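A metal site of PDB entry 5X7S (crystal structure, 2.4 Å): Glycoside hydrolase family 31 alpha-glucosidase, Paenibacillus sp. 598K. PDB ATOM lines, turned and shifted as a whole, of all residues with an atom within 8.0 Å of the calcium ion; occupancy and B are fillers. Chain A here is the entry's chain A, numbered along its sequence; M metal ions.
NH1 of Arg 894 is in salt-bridge range of OD2 of Asp 961, 3.2 Å away.
OE2 of Glu 839 lies close to N of Ser 864 (3.3 Å).
Five residues have an atom within 4 Å of the calcium ion: Glu 837, Glu 839, Ser 862, Gly 865 and Asp 961.
The nearest printed residue that does not touch the calcium ion is Phe 866 (4.3 Å).
The calcium ion is bound by OE1 of Glu 837, OD1 of Asp 961, O of Gly 865, O of Ser 862, O of Asp 961, OE2 of Glu 839 and OE1 of Glu 839.
The calcium ion has seven donor atoms within binding distance.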
ATOM      1  N   GLN A 786      20.909   2.857  38.501  1.00  0.00           N
ATOM      2  CA  GLN A 786      21.936   2.388  37.586  1.00  0.00           C
ATOM      3  C   GLN A 786      22.700   1.156  38.175  1.00  0.00           C
ATOM      4  O   GLN A 786      22.701   0.076  37.550  1.00  0.00           O
ATOM      5  CB  GLN A 786      22.882   3.536  37.137  1.00  0.00           C
ATOM      6  CG  GLN A 786      23.164   3.541  35.629  1.00  0.00           C
ATOM      7  CD  GLN A 786      23.842   2.257  35.145  1.00  0.00           C
ATOM      8  OE1 GLN A 786      25.037   2.044  35.390  1.00  0.00           O
ATOM      9  NE2 GLN A 786      23.090   1.388  34.469  1.00  0.00           N
ATOM     10  N   ILE A 835      18.710  11.882  35.736  1.00  0.00           N
ATOM     11  CA  ILE A 835      19.719  11.476  34.772  1.00  0.00           C
ATOM     12  C   ILE A 835      19.123  10.564  33.682  1.00  0.00           C
ATOM     13  O   ILE A 835      18.533   9.501  33.961  1.00  0.00           O
ATOM     14  CB  ILE A 835      20.959  10.825  35.455  1.00  0.00           C
ATOM     15  CG1 ILE A 835      22.099  10.659  34.438  1.00  0.00           C
ATOM     16  CG2 ILE A 835      20.626   9.493  36.125  1.00  0.00           C
ATOM     17  CD1 ILE A 835      23.457  10.485  35.083  1.00  0.00           C
ATOM     18  N   TYR A 836      19.351  10.972  32.433  1.00  0.00           N
ATOM     19  CA  TYR A 836      18.887  10.209  31.308  1.00  0.00           C
ATOM     20  C   TYR A 836      20.098   9.693  30.519  1.00  0.00           C
ATOM     21  O   TYR A 836      20.779  10.437  29.839  1.00  0.00           O
ATOM     22  CB  TYR A 836      17.920  11.053  30.454  1.00  0.00           C
ATOM     23  CG  TYR A 836      16.675  11.559  31.195  1.00  0.00           C
ATOM     24  CD1 TYR A 836      15.509  10.797  31.291  1.00  0.00           C
ATOM     25  CD2 TYR A 836      16.670  12.831  31.760  1.00  0.00           C
ATOM     26  CE1 TYR A 836      14.388  11.274  31.999  1.00  0.00           C
ATOM     27  CE2 TYR A 836      15.577  13.314  32.446  1.00  0.00           C
ATOM     28  CZ  TYR A 836      14.447  12.535  32.557  1.00  0.00           C
ATOM     29  OH  TYR A 836      13.400  13.098  33.221  1.00  0.00           O
ATOM     30  N   GLU A 837      20.319   8.389  30.588  1.00  0.00           N
ATOM     31  CA  GLU A 837      21.269   7.728  29.728  1.00  0.00           C
ATOM     32  C   GLU A 837      20.764   7.654  28.275  1.00  0.00           C
ATOM     33  O   GLU A 837      19.844   6.889  27.985  1.00  0.00           O
ATOM     34  CB  GLU A 837      21.611   6.339  30.263  1.00  0.00           C
ATOM     35  CG  GLU A 837      22.284   6.338  31.648  1.00  0.00           C
ATOM     36  CD  GLU A 837      23.667   7.006  31.726  1.00  0.00           C
ATOM     37  OE1 GLU A 837      24.303   7.266  30.675  1.00  0.00           O
ATOM     38  OE2 GLU A 837      24.123   7.290  32.863  1.00  0.00           O
ATOM     39  N   VAL A 838      21.412   8.424  27.377  1.00  0.00           N
ATOM     40  CA  VAL A 838      20.964   8.585  25.986  1.00  0.00           C
ATOM     41  C   VAL A 838      20.990   7.312  25.182  1.00  0.00           C
ATOM     42  O   VAL A 838      20.211   7.177  24.235  1.00  0.00           O
ATOM     43  CB  VAL A 838      21.689   9.712  25.201  1.00  0.00           C
ATOM     44  CG1 VAL A 838      21.311  11.089  25.764  1.00  0.00           C
ATOM     45  CG2 VAL A 838      23.197   9.541  25.191  1.00  0.00           C
ATOM     46  N   GLU A 839      21.835   6.358  25.560  1.00  0.00           N
ATOM     47  CA  GLU A 839      21.810   5.018  24.930  1.00  0.00           C
ATOM     48  C   GLU A 839      20.512   4.257  25.170  1.00  0.00           C
ATOM     49  O   GLU A 839      20.188   3.375  24.402  1.00  0.00           O
ATOM     50  CB  GLU A 839      23.019   4.152  25.366  1.00  0.00           C
ATOM     51  CG  GLU A 839      23.105   3.751  26.850  1.00  0.00           C
ATOM     52  CD  GLU A 839      23.776   4.784  27.726  1.00  0.00           C
ATOM     53  OE1 GLU A 839      23.756   5.998  27.343  1.00  0.00           O
ATOM     54  OE2 GLU A 839      24.291   4.407  28.812  1.00  0.00           O
ATOM     55  N   ASP A 840      19.806   4.583  26.257  1.00  0.00           N
ATOM     56  CA  ASP A 840      18.436   4.141  26.462  1.00  0.00           C
ATOM     57  C   ASP A 840      17.354   5.053  25.764  1.00  0.00           C
ATOM     58  O   ASP A 840      16.204   4.659  25.666  1.00  0.00           O
ATOM     59  CB  ASP A 840      18.134   4.028  27.980  1.00  0.00           C
ATOM     60  CG  ASP A 840      19.051   3.007  28.718  1.00  0.00           C
ATOM     61  OD1 ASP A 840      19.673   2.117  28.061  1.00  0.00           O
ATOM     62  OD2 ASP A 840      19.129   3.103  29.961  1.00  0.00           O
ATOM     63  N   ASN A 855      27.129   2.411  21.602  1.00  0.00           N
ATOM     64  CA  ASN A 855      28.419   1.728  21.697  1.00  0.00           C
ATOM     65  C   ASN A 855      29.026   1.745  23.101  1.00  0.00           C
ATOM     66  O   ASN A 855      28.622   2.539  23.969  1.00  0.00           O
ATOM     67  CB  ASN A 855      29.423   2.308  20.669  1.00  0.00           C
ATOM     68  CG  ASN A 855      30.159   1.209  19.884  1.00  0.00           C
ATOM     69  OD1 ASN A 855      30.597   0.219  20.447  1.00  0.00           O
ATOM     70  ND2 ASN A 855      30.310   1.418  18.579  1.00  0.00           N
ATOM     71  N   GLY A 860      35.223   5.371  29.965  1.00  0.00           N
ATOM     72  CA  GLY A 860      34.849   6.576  30.733  1.00  0.00           C
ATOM     73  C   GLY A 860      33.350   6.930  30.764  1.00  0.00           C
ATOM     74  O   GLY A 860      32.948   7.897  31.436  1.00  0.00           O
ATOM     75  N   TYR A 861      32.532   6.144  30.057  1.00  0.00           N
ATOM     76  CA  TYR A 861      31.093   6.377  29.944  1.00  0.00           C
ATOM     77  C   TYR A 861      30.368   5.958  31.202  1.00  0.00           C
ATOM     78  O   TYR A 861      30.835   5.049  31.927  1.00  0.00           O
ATOM     79  CB  TYR A 861      30.487   5.649  28.740  1.00  0.00           C
ATOM     80  CG  TYR A 861      30.644   4.131  28.747  1.00  0.00           C
ATOM     81  CD1 TYR A 861      29.765   3.324  29.456  1.00  0.00           C
ATOM     82  CD2 TYR A 861      31.690   3.509  28.022  1.00  0.00           C
ATOM     83  CE1 TYR A 861      29.924   1.926  29.451  1.00  0.00           C
ATOM     84  CE2 TYR A 861      31.853   2.124  27.999  1.00  0.00           C
ATOM     85  CZ  TYR A 861      30.963   1.326  28.727  1.00  0.00           C
ATOM     86  OH  TYR A 861      31.051  -0.051  28.757  1.00  0.00           O
ATOM     87  N   SER A 862      29.233   6.628  31.447  1.00  0.00           N
ATOM     88  CA  SER A 862      28.207   6.242  32.440  1.00  0.00           C
ATOM     89  C   SER A 862      27.163   5.263  31.870  1.00  0.00           C
ATOM     90  O   SER A 862      26.834   5.261  30.675  1.00  0.00           O
ATOM     91  CB  SER A 862      27.491   7.487  32.971  1.00  0.00           C
ATOM     92  OG  SER A 862      26.467   7.148  33.892  1.00  0.00           O
ATOM     93  N   GLY A 863      26.594   4.439  32.734  1.00  0.00           N
ATOM     94  CA  GLY A 863      25.620   3.465  32.262  1.00  0.00           C
ATOM     95  C   GLY A 863      26.206   2.351  31.400  1.00  0.00           C
ATOM     96  O   GLY A 863      27.391   1.963  31.575  1.00  0.00           O
ATOM     97  N   SER A 864      25.377   1.825  30.502  1.00  0.00           N
ATOM     98  CA  SER A 864      25.735   0.679  29.697  1.00  0.00           C
ATOM     99  C   SER A 864      26.388   1.123  28.399  1.00  0.00           C
ATOM    100  O   SER A 864      26.793   0.262  27.618  1.00  0.00           O
ATOM    101  CB  SER A 864      24.491  -0.164  29.405  1.00  0.00           C
ATOM    102  OG  SER A 864      23.526   0.592  28.691  1.00  0.00           O
ATOM    103  N   GLY A 865      26.524   2.435  28.172  1.00  0.00           N
ATOM    104  CA  GLY A 865      27.199   2.917  26.988  1.00  0.00           C
ATOM    105  C   GLY A 865      27.076   4.412  26.687  1.00  0.00           C
ATOM    106  O   GLY A 865      27.022   5.252  27.583  1.00  0.00           O
ATOM    107  N   PHE A 866      27.056   4.733  25.420  1.00  0.00           N
ATOM    108  CA  PHE A 866      26.897   6.088  24.948  1.00  0.00           C
ATOM    109  C   PHE A 866      26.328   6.014  23.528  1.00  0.00           C
ATOM    110  O   PHE A 866      26.144   4.927  22.961  1.00  0.00           O
ATOM    111  CB  PHE A 866      28.228   6.816  24.976  1.00  0.00           C
ATOM    112  CG  PHE A 866      29.329   6.086  24.258  1.00  0.00           C
ATOM    113  CD1 PHE A 866      29.529   6.262  22.900  1.00  0.00           C
ATOM    114  CD2 PHE A 866      30.154   5.201  24.947  1.00  0.00           C
ATOM    115  CE1 PHE A 866      30.541   5.568  22.237  1.00  0.00           C
ATOM    116  CE2 PHE A 866      31.165   4.516  24.297  1.00  0.00           C
ATOM    117  CZ  PHE A 866      31.358   4.699  22.942  1.00  0.00           C
ATOM    118  N   VAL A 867      26.081   7.154  22.949  1.00  0.00           N
ATOM    119  CA  VAL A 867      25.462   7.221  21.649  1.00  0.00           C
ATOM    120  C   VAL A 867      26.519   7.723  20.648  1.00  0.00           C
ATOM    121  O   VAL A 867      27.156   8.753  20.889  1.00  0.00           O
ATOM    122  CB  VAL A 867      24.214   8.118  21.731  1.00  0.00           C
ATOM    123  CG1 VAL A 867      23.833   8.677  20.378  1.00  0.00           C
ATOM    124  CG2 VAL A 867      23.079   7.319  22.384  1.00  0.00           C
ATOM    125  N   ARG A 894      26.505  15.244  28.728  1.00  0.00           N
ATOM    126  CA  ARG A 894      27.829  14.638  28.846  1.00  0.00           C
ATOM    127  C   ARG A 894      28.259  14.048  27.509  1.00  0.00           C
ATOM    128  O   ARG A 894      27.625  13.092  27.015  1.00  0.00           O
ATOM    129  CB  ARG A 894      27.929  13.594  29.959  1.00  0.00           C
ATOM    130  CG  ARG A 894      29.380  13.153  30.216  1.00  0.00           C
ATOM    131  CD  ARG A 894      29.768  13.232  31.676  1.00  0.00           C
ATOM    132  NE  ARG A 894      31.161  12.950  32.031  1.00  0.00           N
ATOM    133  CZ  ARG A 894      31.739  11.737  31.977  1.00  0.00           C
ATOM    134  NH1 ARG A 894      31.110  10.645  31.481  1.00  0.00           N
ATOM    135  NH2 ARG A 894      33.004  11.616  32.380  1.00  0.00           N
ATOM    136  N   TRP A 928      35.771  12.658  28.624  1.00  0.00           N
ATOM    137  CA  TRP A 928      34.394  13.218  28.566  1.00  0.00           C
ATOM    138  C   TRP A 928      34.281  14.610  29.185  1.00  0.00           C
ATOM    139  O   TRP A 928      34.948  14.922  30.141  1.00  0.00           O
ATOM    140  CB  TRP A 928      33.416  12.273  29.260  1.00  0.00           C
ATOM    141  CG  TRP A 928      33.440  10.908  28.686  1.00  0.00           C
ATOM    142  CD1 TRP A 928      34.305   9.904  28.997  1.00  0.00           C
ATOM    143  CD2 TRP A 928      32.564  10.378  27.672  1.00  0.00           C
ATOM    144  NE1 TRP A 928      34.024   8.785  28.245  1.00  0.00           N
ATOM    145  CE2 TRP A 928      32.959   9.045  27.425  1.00  0.00           C
ATOM    146  CE3 TRP A 928      31.473  10.899  26.945  1.00  0.00           C
ATOM    147  CZ2 TRP A 928      32.321   8.228  26.483  1.00  0.00           C
ATOM    148  CZ3 TRP A 928      30.834  10.099  26.026  1.00  0.00           C
ATOM    149  CH2 TRP A 928      31.270   8.765  25.799  1.00  0.00           C
ATOM    150  N   LEU A 960      27.688  10.908  22.742  1.00  0.00           N
ATOM    151  CA  LEU A 960      26.855  11.440  23.842  1.00  0.00           C
ATOM    152  C   LEU A 960      26.623  10.414  24.915  1.00  0.00           C
ATOM    153  O   LEU A 960      26.261   9.262  24.613  1.00  0.00           O
ATOM    154  CB  LEU A 960      25.524  11.945  23.301  1.00  0.00           C
ATOM    155  CG  LEU A 960      25.589  13.117  22.294  1.00  0.00           C
ATOM    156  CD1 LEU A 960      24.169  13.677  22.055  1.00  0.00           C
ATOM    157  CD2 LEU A 960      26.568  14.231  22.686  1.00  0.00           C
ATOM    158  N   ASP A 961      26.870  10.788  26.159  1.00  0.00           N
ATOM    159  CA  ASP A 961      26.796   9.821  27.257  1.00  0.00           C
ATOM    160  C   ASP A 961      25.484   9.863  27.986  1.00  0.00           C
ATOM    161  O   ASP A 961      24.906   8.794  28.270  1.00  0.00           O
ATOM    162  CB  ASP A 961      27.899  10.037  28.293  1.00  0.00           C
ATOM    163  CG  ASP A 961      27.996   8.864  29.247  1.00  0.00           C
ATOM    164  OD1 ASP A 961      27.337   7.820  28.963  1.00  0.00           O
ATOM    165  OD2 ASP A 961      28.698   8.970  30.293  1.00  0.00           O
ATOM    166  N   TYR A 962      25.047  11.079  28.348  1.00  0.00           N
ATOM    167  CA  TYR A 962      23.780  11.283  29.089  1.00  0.00           C
ATOM    168  C   TYR A 962      23.433  12.727  29.181  1.00  0.00           C
ATOM    169  O   TYR A 962      24.291  13.556  28.918  1.00  0.00           O
ATOM    170  CB  TYR A 962      23.836  10.745  30.533  1.00  0.00           C
ATOM    171  CG  TYR A 962      24.904  11.393  31.449  1.00  0.00           C
ATOM    172  CD1 TYR A 962      24.773  12.715  31.933  1.00  0.00           C
ATOM    173  CD2 TYR A 962      26.022  10.656  31.889  1.00  0.00           C
ATOM    174  CE1 TYR A 962      25.741  13.300  32.759  1.00  0.00           C
ATOM    175  CE2 TYR A 962      26.991  11.230  32.740  1.00  0.00           C
ATOM    176  CZ  TYR A 962      26.842  12.544  33.176  1.00  0.00           C
ATOM    177  OH  TYR A 962      27.782  13.119  33.999  1.00  0.00           O
ATOM    178  N   ILE A 963      22.196  13.024  29.583  1.00  0.00           N
ATOM    179  CA  ILE A 963      21.884  14.362  30.081  1.00  0.00           C
ATOM    180  C   ILE A 963      21.349  14.330  31.489  1.00  0.00           C
ATOM    181  O   ILE A 963      20.858  13.286  31.955  1.00  0.00           O
ATOM    182  CB  ILE A 963      20.920  15.157  29.185  1.00  0.00           C
ATOM    183  CG1 ILE A 963      19.518  14.517  29.166  1.00  0.00           C
ATOM    184  CG2 ILE A 963      21.510  15.308  27.778  1.00  0.00           C
ATOM    185  CD1 ILE A 963      18.471  15.440  28.577  1.00  0.00           C
HETATM  186 CA    CA M   1      25.547   6.534  29.009  1.00  0.00          CA
